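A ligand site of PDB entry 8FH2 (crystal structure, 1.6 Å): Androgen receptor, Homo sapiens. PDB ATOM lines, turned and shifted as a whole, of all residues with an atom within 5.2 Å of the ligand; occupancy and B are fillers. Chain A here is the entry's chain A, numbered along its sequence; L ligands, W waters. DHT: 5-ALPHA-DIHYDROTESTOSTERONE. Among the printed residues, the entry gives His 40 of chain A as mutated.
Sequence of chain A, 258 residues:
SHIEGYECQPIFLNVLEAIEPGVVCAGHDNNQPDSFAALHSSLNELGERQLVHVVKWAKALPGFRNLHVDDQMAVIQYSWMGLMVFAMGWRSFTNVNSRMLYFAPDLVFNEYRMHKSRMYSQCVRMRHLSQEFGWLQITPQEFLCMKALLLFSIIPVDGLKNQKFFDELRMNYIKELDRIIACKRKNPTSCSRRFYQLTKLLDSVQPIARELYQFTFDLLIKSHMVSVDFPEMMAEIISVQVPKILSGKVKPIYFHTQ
An oxygen (O17) of the ligand lies within hydrogen-bond range of the side-chain hydroxyl (OG1) of Thr 216 (2.7 Å).
An oxygen (O17) of the ligand sits at hydrogen-bond distance from the side-chain amide oxygen of Asn 44 (2.8 Å).
O3 of the ligand sits at hydrogen-bond distance from NH2 of Arg 91 (2.9 Å).
The backbone carbonyl oxygen (O) of His 40 sits close to the side-chain amide nitrogen (ND2) of Asn 44 (3.3 Å).
NE2 of Gln 50 lies close to NH2 of Arg 91, 3.3 Å away.
O of Phe 103 lies within hydrogen-bond range of NH2 of Arg 91, 2.9 Å away.
The side-chain amide oxygen (OE1) of Gln 50 lies close to the side-chain sulfur (SD) of Met 84, at 3.8 Å.
Leu 43 touches the ligand (O to C11, 3.4 Å).
Leu 46 touches the ligand (CD2 to C2, 3.7 Å).
OE1 of Gln 50 touches C2 of the ligand, 3.3 Å away.
Met 81 touches the ligand (CE to C18, 3.8 Å).
SD of Met 84 touches C19 of the ligand, 3.7 Å away.
CB of Met 88 touches O3 of the ligand (3.6 Å).
Phe 103 touches the ligand.
Met 119 touches the ligand.
CD1 of Phe 215 touches C16 of the ligand, 3.9 Å away.
Phe 230 touches the ligand.
Met 234 touches the ligand.
Hydrophobic or aromatic side chains within 4 Å of the ligand: Leu 43, Leu 46, Met 81, Met 84, Met 88, Phe 103, Met 119, Phe 215, Phe 230 and Met 234.
Within 4 Å of the ligand: Leu 43, Asn 44, Leu 46, Gln 50, Met 81, Met 84, Met 88, Arg 91, Phe 103, Met 119, Phe 215, Thr 216, Phe 230 and Met 234.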
ATOM      1  N   HIS A  40      25.711  -8.085 -29.515  1.00  0.00           N
ATOM      2  CA  HIS A  40      26.653  -7.561 -28.533  1.00  0.00           C
ATOM      3  C   HIS A  40      28.086  -7.901 -28.881  1.00  0.00           C
ATOM      4  O   HIS A  40      28.982  -7.109 -28.556  1.00  0.00           O
ATOM      5  CB  HIS A  40      26.280  -8.056 -27.138  1.00  0.00           C
ATOM      6  CG  HIS A  40      25.110  -7.327 -26.585  1.00  0.00           C
ATOM      7  ND1 HIS A  40      25.153  -5.979 -26.329  1.00  0.00           N
ATOM      8  CD2 HIS A  40      23.841  -7.731 -26.327  1.00  0.00           C
ATOM      9  CE1 HIS A  40      23.958  -5.576 -25.915  1.00  0.00           C
ATOM     10  NE2 HIS A  40      23.155  -6.626 -25.890  1.00  0.00           N
ATOM     11  N   LEU A  43      28.825  -5.070 -31.123  1.00  0.00           N
ATOM     12  CA  LEU A  43      28.970  -3.808 -30.402  1.00  0.00           C
ATOM     13  C   LEU A  43      30.286  -3.773 -29.640  1.00  0.00           C
ATOM     14  O   LEU A  43      30.960  -2.729 -29.591  1.00  0.00           O
ATOM     15  CB  LEU A  43      27.807  -3.578 -29.430  1.00  0.00           C
ATOM     16  CG  LEU A  43      26.486  -3.129 -30.053  1.00  0.00           C
ATOM     17  CD1 LEU A  43      25.347  -3.257 -29.059  1.00  0.00           C
ATOM     18  CD2 LEU A  43      26.571  -1.707 -30.600  1.00  0.00           C
ATOM     19  N   ASN A  44      30.704  -4.912 -29.069  1.00  0.00           N
ATOM     20  CA  ASN A  44      31.943  -4.928 -28.301  1.00  0.00           C
ATOM     21  C   ASN A  44      33.140  -4.717 -29.209  1.00  0.00           C
ATOM     22  O   ASN A  44      34.076  -3.997 -28.848  1.00  0.00           O
ATOM     23  CB  ASN A  44      32.098  -6.249 -27.556  1.00  0.00           C
ATOM     24  CG  ASN A  44      31.171  -6.350 -26.390  1.00  0.00           C
ATOM     25  OD1 ASN A  44      30.743  -5.333 -25.851  1.00  0.00           O
ATOM     26  ND2 ASN A  44      30.927  -7.576 -25.924  1.00  0.00           N
ATOM     27  N   LEU A  46      33.081  -3.056 -31.997  1.00  0.00           N
ATOM     28  CA  LEU A  46      33.064  -1.634 -32.338  1.00  0.00           C
ATOM     29  C   LEU A  46      33.629  -0.791 -31.211  1.00  0.00           C
ATOM     30  O   LEU A  46      34.397   0.146 -31.437  1.00  0.00           O
ATOM     31  CB  LEU A  46      31.636  -1.203 -32.719  1.00  0.00           C
ATOM     32  CG  LEU A  46      31.462   0.292 -32.924  1.00  0.00           C
ATOM     33  CD1 LEU A  46      32.066   0.639 -34.288  1.00  0.00           C
ATOM     34  CD2 LEU A  46      29.970   0.596 -33.016  1.00  0.00           C
ATOM     35  N   GLY A  47      33.285  -1.128 -29.958  1.00  0.00           N
ATOM     36  CA  GLY A  47      33.882  -0.427 -28.847  1.00  0.00           C
ATOM     37  C   GLY A  47      35.397  -0.528 -28.829  1.00  0.00           C
ATOM     38  O   GLY A  47      36.087   0.458 -28.549  1.00  0.00           O
ATOM     39  N   GLN A  50      36.701   1.684 -31.598  1.00  0.00           N
ATOM     40  CA  GLN A  50      36.536   3.092 -31.291  1.00  0.00           C
ATOM     41  C   GLN A  50      37.453   3.537 -30.151  1.00  0.00           C
ATOM     42  O   GLN A  50      37.856   4.696 -30.097  1.00  0.00           O
ATOM     43  CB  GLN A  50      35.065   3.360 -30.926  1.00  0.00           C
ATOM     44  CG  GLN A  50      34.117   3.293 -32.145  1.00  0.00           C
ATOM     45  CD  GLN A  50      32.814   4.040 -31.935  1.00  0.00           C
ATOM     46  OE1 GLN A  50      32.628   4.710 -30.930  1.00  0.00           O
ATOM     47  NE2 GLN A  50      31.901   3.903 -32.883  1.00  0.00           N
ATOM     48  N   TRP A  80      35.127   7.216 -21.661  1.00  0.00           N
ATOM     49  CA  TRP A  80      34.926   6.667 -23.012  1.00  0.00           C
ATOM     50  C   TRP A  80      33.448   6.396 -23.344  1.00  0.00           C
ATOM     51  O   TRP A  80      33.021   6.650 -24.473  1.00  0.00           O
ATOM     52  CB  TRP A  80      35.784   5.423 -23.196  1.00  0.00           C
ATOM     53  CG  TRP A  80      35.418   4.266 -22.326  1.00  0.00           C
ATOM     54  CD1 TRP A  80      35.943   4.009 -21.080  1.00  0.00           C
ATOM     55  CD2 TRP A  80      34.576   3.155 -22.628  1.00  0.00           C
ATOM     56  NE1 TRP A  80      35.419   2.850 -20.576  1.00  0.00           N
ATOM     57  CE2 TRP A  80      34.590   2.289 -21.511  1.00  0.00           C
ATOM     58  CE3 TRP A  80      33.786   2.813 -23.734  1.00  0.00           C
ATOM     59  CZ2 TRP A  80      33.857   1.114 -21.459  1.00  0.00           C
ATOM     60  CZ3 TRP A  80      33.059   1.618 -23.687  1.00  0.00           C
ATOM     61  CH2 TRP A  80      33.096   0.795 -22.548  1.00  0.00           C
ATOM     62  N   MET A  81      32.674   5.871 -22.403  1.00  0.00           N
ATOM     63  CA  MET A  81      31.303   5.492 -22.741  1.00  0.00           C
ATOM     64  C   MET A  81      30.523   6.753 -23.118  1.00  0.00           C
ATOM     65  O   MET A  81      29.805   6.804 -24.124  1.00  0.00           O
ATOM     66  CB  MET A  81      30.631   4.848 -21.525  1.00  0.00           C
ATOM     67  CG  MET A  81      29.242   4.254 -21.667  1.00  0.00           C
ATOM     68  SD  MET A  81      29.078   3.022 -22.974  1.00  0.00           S
ATOM     69  CE  MET A  81      29.570   1.681 -21.898  1.00  0.00           C
ATOM     70  N   MET A  84      31.674   8.095 -26.506  1.00  0.00           N
ATOM     71  CA  MET A  84      31.208   7.348 -27.667  1.00  0.00           C
ATOM     72  C   MET A  84      29.702   7.449 -27.843  1.00  0.00           C
ATOM     73  O   MET A  84      29.213   7.420 -28.973  1.00  0.00           O
ATOM     74  CB  MET A  84      31.550   5.856 -27.690  1.00  0.00           C
ATOM     75  CG  MET A  84      33.030   5.512 -27.901  1.00  0.00           C
ATOM     76  SD  MET A  84      33.478   3.854 -27.333  1.00  0.00           S
ATOM     77  CE  MET A  84      35.274   3.922 -27.398  1.00  0.00           C
ATOM     78  N   VAL A  85      28.943   7.553 -26.755  1.00  0.00           N
ATOM     79  CA  VAL A  85      27.486   7.655 -26.902  1.00  0.00           C
ATOM     80  C   VAL A  85      27.122   9.019 -27.481  1.00  0.00           C
ATOM     81  O   VAL A  85      26.243   9.127 -28.350  1.00  0.00           O
ATOM     82  CB  VAL A  85      26.817   7.411 -25.537  1.00  0.00           C
ATOM     83  CG1 VAL A  85      25.410   8.038 -25.469  1.00  0.00           C
ATOM     84  CG2 VAL A  85      26.840   5.928 -25.185  1.00  0.00           C
ATOM     85  N   MET A  88      27.925   8.918 -31.146  1.00  0.00           N
ATOM     86  CA  MET A  88      26.932   8.097 -31.828  1.00  0.00           C
ATOM     87  C   MET A  88      25.617   8.833 -31.980  1.00  0.00           C
ATOM     88  O   MET A  88      24.956   8.738 -33.027  1.00  0.00           O
ATOM     89  CB  MET A  88      26.769   6.772 -31.065  1.00  0.00           C
ATOM     90  CG  MET A  88      25.852   5.741 -31.720  1.00  0.00           C
ATOM     91  SD  MET A  88      24.086   6.027 -31.413  1.00  0.00           S
ATOM     92  CE  MET A  88      24.047   5.821 -29.622  1.00  0.00           C
ATOM     93  N   ARG A  91      26.089  11.131 -34.951  1.00  0.00           N
ATOM     94  CA  ARG A  91      26.039  10.327 -36.181  1.00  0.00           C
ATOM     95  C   ARG A  91      24.600   9.996 -36.521  1.00  0.00           C
ATOM     96  O   ARG A  91      24.180  10.065 -37.688  1.00  0.00           O
ATOM     97  CB  ARG A  91      26.815   9.029 -35.987  1.00  0.00           C
ATOM     98  CG  ARG A  91      28.317   9.090 -36.122  1.00  0.00           C
ATOM     99  CD  ARG A  91      28.877   7.695 -36.387  1.00  0.00           C
ATOM    100  NE  ARG A  91      28.725   6.731 -35.300  1.00  0.00           N
ATOM    101  CZ  ARG A  91      29.375   6.762 -34.140  1.00  0.00           C
ATOM    102  NH1 ARG A  91      30.171   7.768 -33.803  1.00  0.00           N
ATOM    103  NH2 ARG A  91      29.225   5.731 -33.299  1.00  0.00           N
ATOM    104  N   PHE A 103      25.145   3.177 -34.873  1.00  0.00           N
ATOM    105  CA  PHE A 103      26.377   2.820 -34.166  1.00  0.00           C
ATOM    106  C   PHE A 103      27.547   2.829 -35.128  1.00  0.00           C
ATOM    107  O   PHE A 103      28.638   3.315 -34.820  1.00  0.00           O
ATOM    108  CB  PHE A 103      26.251   1.451 -33.504  1.00  0.00           C
ATOM    109  CG  PHE A 103      25.275   1.428 -32.352  1.00  0.00           C
ATOM    110  CD1 PHE A 103      25.636   1.970 -31.128  1.00  0.00           C
ATOM    111  CD2 PHE A 103      24.055   0.764 -32.446  1.00  0.00           C
ATOM    112  CE1 PHE A 103      24.761   1.941 -30.059  1.00  0.00           C
ATOM    113  CE2 PHE A 103      23.172   0.715 -31.367  1.00  0.00           C
ATOM    114  CZ  PHE A 103      23.531   1.296 -30.174  1.00  0.00           C
ATOM    115  N   MET A 119      18.519  -4.368 -24.584  1.00  0.00           N
ATOM    116  CA  MET A 119      18.815  -3.055 -24.014  1.00  0.00           C
ATOM    117  C   MET A 119      17.967  -1.982 -24.698  1.00  0.00           C
ATOM    118  O   MET A 119      18.406  -0.873 -24.988  1.00  0.00           O
ATOM    119  CB  MET A 119      20.337  -2.865 -24.010  1.00  0.00           C
ATOM    120  CG  MET A 119      20.985  -2.396 -25.238  1.00  0.00           C
ATOM    121  SD  MET A 119      22.745  -1.966 -25.017  1.00  0.00           S
ATOM    122  CE  MET A 119      23.005  -1.323 -26.667  1.00  0.00           C
ATOM    123  N   MET A 126      19.231   6.751 -25.485  1.00  0.00           N
ATOM    124  CA  MET A 126      20.234   7.181 -26.469  1.00  0.00           C
ATOM    125  C   MET A 126      19.570   7.865 -27.656  1.00  0.00           C
ATOM    126  O   MET A 126      20.113   8.834 -28.206  1.00  0.00           O
ATOM    127  CB  MET A 126      21.016   5.947 -26.916  1.00  0.00           C
ATOM    128  CG  MET A 126      21.962   5.434 -25.848  1.00  0.00           C
ATOM    129  SD  MET A 126      23.281   4.376 -26.467  1.00  0.00           S
ATOM    130  CE  MET A 126      22.384   2.826 -26.581  1.00  0.00           C
ATOM    131  N   LEU A 212      24.619   2.304 -19.280  1.00  0.00           N
ATOM    132  CA  LEU A 212      25.326   1.399 -20.169  1.00  0.00           C
ATOM    133  C   LEU A 212      26.496   0.733 -19.476  1.00  0.00           C
ATOM    134  O   LEU A 212      26.805  -0.429 -19.754  1.00  0.00           O
ATOM    135  CB  LEU A 212      25.793   2.135 -21.430  1.00  0.00           C
ATOM    136  CG  LEU A 212      24.632   2.670 -22.258  1.00  0.00           C
ATOM    137  CD1 LEU A 212      25.089   3.802 -23.202  1.00  0.00           C
ATOM    138  CD2 LEU A 212      23.955   1.540 -22.965  1.00  0.00           C
ATOM    139  N   PHE A 215      25.090  -2.089 -17.644  1.00  0.00           N
ATOM    140  CA  PHE A 215      24.706  -3.166 -18.535  1.00  0.00           C
ATOM    141  C   PHE A 215      25.919  -3.940 -19.010  1.00  0.00           C
ATOM    142  O   PHE A 215      25.911  -5.177 -19.029  1.00  0.00           O
ATOM    143  CB  PHE A 215      23.911  -2.565 -19.699  1.00  0.00           C
ATOM    144  CG  PHE A 215      23.335  -3.591 -20.648  1.00  0.00           C
ATOM    145  CD1 PHE A 215      24.093  -4.126 -21.662  1.00  0.00           C
ATOM    146  CD2 PHE A 215      22.008  -3.987 -20.518  1.00  0.00           C
ATOM    147  CE1 PHE A 215      23.555  -5.059 -22.543  1.00  0.00           C
ATOM    148  CE2 PHE A 215      21.462  -4.900 -21.407  1.00  0.00           C
ATOM    149  CZ  PHE A 215      22.239  -5.433 -22.410  1.00  0.00           C
ATOM    150  N   THR A 216      26.981  -3.235 -19.436  1.00  0.00           N
ATOM    151  CA  THR A 216      28.124  -3.961 -19.977  1.00  0.00           C
ATOM    152  C   THR A 216      28.885  -4.717 -18.883  1.00  0.00           C
ATOM    153  O   THR A 216      29.440  -5.781 -19.149  1.00  0.00           O
ATOM    154  CB  THR A 216      29.046  -3.009 -20.760  1.00  0.00           C
ATOM    155  OG1 THR A 216      29.943  -3.786 -21.553  1.00  0.00           O
ATOM    156  CG2 THR A 216      29.884  -2.103 -19.835  1.00  0.00           C
ATOM    157  N   LEU A 219      26.979  -7.829 -18.405  1.00  0.00           N
ATOM    158  CA  LEU A 219      27.129  -8.691 -19.563  1.00  0.00           C
ATOM    159  C   LEU A 219      28.498  -9.366 -19.550  1.00  0.00           C
ATOM    160  O   LEU A 219      28.620 -10.537 -19.876  1.00  0.00           O
ATOM    161  CB  LEU A 219      26.928  -7.870 -20.845  1.00  0.00           C
ATOM    162  CG  LEU A 219      27.035  -8.567 -22.196  1.00  0.00           C
ATOM    163  CD1 LEU A 219      26.136  -9.810 -22.246  1.00  0.00           C
ATOM    164  CD2 LEU A 219      26.699  -7.602 -23.307  1.00  0.00           C
ATOM    165  N   PHE A 230      34.126 -10.577 -25.583  1.00  0.00           N
ATOM    166  CA  PHE A 230      34.661  -9.267 -25.242  1.00  0.00           C
ATOM    167  C   PHE A 230      36.109  -9.188 -25.686  1.00  0.00           C
ATOM    168  O   PHE A 230      36.944  -9.981 -25.220  1.00  0.00           O
ATOM    169  CB  PHE A 230      34.574  -8.986 -23.737  1.00  0.00           C
ATOM    170  CG  PHE A 230      33.229  -8.501 -23.267  1.00  0.00           C
ATOM    171  CD1 PHE A 230      32.190  -9.388 -23.082  1.00  0.00           C
ATOM    172  CD2 PHE A 230      33.000  -7.143 -23.034  1.00  0.00           C
ATOM    173  CE1 PHE A 230      30.950  -8.959 -22.643  1.00  0.00           C
ATOM    174  CE2 PHE A 230      31.760  -6.714 -22.595  1.00  0.00           C
ATOM    175  CZ  PHE A 230      30.735  -7.615 -22.396  1.00  0.00           C
ATOM    176  N   MET A 234      38.499  -3.987 -24.001  1.00  0.00           N
ATOM    177  CA  MET A 234      37.180  -3.836 -23.382  1.00  0.00           C
ATOM    178  C   MET A 234      37.083  -4.670 -22.112  1.00  0.00           C
ATOM    179  O   MET A 234      36.591  -4.187 -21.098  1.00  0.00           O
ATOM    180  CB  MET A 234      36.065  -4.217 -24.352  1.00  0.00           C
ATOM    181  CG  MET A 234      35.984  -3.284 -25.586  1.00  0.00           C
ATOM    182  SD  MET A 234      35.105  -1.767 -25.191  1.00  0.00           S
ATOM    183  CE  MET A 234      33.413  -2.370 -25.158  1.00  0.00           C
ATOM    184  N   ILE A 238      36.489  -2.851 -18.551  1.00  0.00           N
ATOM    185  CA  ILE A 238      35.198  -3.053 -17.904  1.00  0.00           C
ATOM    186  C   ILE A 238      35.341  -3.794 -16.576  1.00  0.00           C
ATOM    187  O   ILE A 238      34.482  -3.649 -15.701  1.00  0.00           O
ATOM    188  CB  ILE A 238      34.243  -3.769 -18.863  1.00  0.00           C
ATOM    189  CG1 ILE A 238      33.948  -2.821 -20.035  1.00  0.00           C
ATOM    190  CG2 ILE A 238      32.959  -4.187 -18.144  1.00  0.00           C
ATOM    191  CD1 ILE A 238      33.265  -3.513 -21.216  1.00  0.00           C
HETATM  192  C1  DHT L   1      30.094   1.232 -29.111  1.00  0.00           C
HETATM  193  C2  DHT L   1      30.348   2.528 -29.863  1.00  0.00           C
HETATM  194  C3  DHT L   1      29.128   3.369 -30.034  1.00  0.00           C
HETATM  195  O3  DHT L   1      28.826   3.868 -31.096  1.00  0.00           O
HETATM  196  C4  DHT L   1      28.261   3.523 -28.808  1.00  0.00           C
HETATM  197  C5  DHT L   1      27.990   2.153 -28.178  1.00  0.00           C
HETATM  198  C6  DHT L   1      27.138   2.318 -26.925  1.00  0.00           C
HETATM  199  C7  DHT L   1      26.804   0.949 -26.330  1.00  0.00           C
HETATM  200  C8  DHT L   1      28.051   0.150 -25.973  1.00  0.00           C
HETATM  201  C9  DHT L   1      28.949   0.035 -27.212  1.00  0.00           C
HETATM  202  C10 DHT L   1      29.306   1.422 -27.798  1.00  0.00           C
HETATM  203  C11 DHT L   1      30.198  -0.789 -26.853  1.00  0.00           C
HETATM  204  C12 DHT L   1      29.857  -2.174 -26.320  1.00  0.00           C
HETATM  205  C13 DHT L   1      28.867  -2.107 -25.144  1.00  0.00           C
HETATM  206  C14 DHT L   1      27.657  -1.274 -25.602  1.00  0.00           C
HETATM  207  C15 DHT L   1      26.666  -1.479 -24.449  1.00  0.00           C
HETATM  208  C16 DHT L   1      26.902  -2.944 -24.018  1.00  0.00           C
HETATM  209  C17 DHT L   1      28.128  -3.425 -24.816  1.00  0.00           C
HETATM  210  O17 DHT L   1      28.905  -4.290 -23.981  1.00  0.00           O
HETATM  211  C18 DHT L   1      29.570  -1.557 -23.885  1.00  0.00           C
HETATM  212  C19 DHT L   1      30.161   2.250 -26.827  1.00  0.00           C
HETATM  213  O   HOH W   1      30.902   6.561 -31.124  1.00  0.00           O
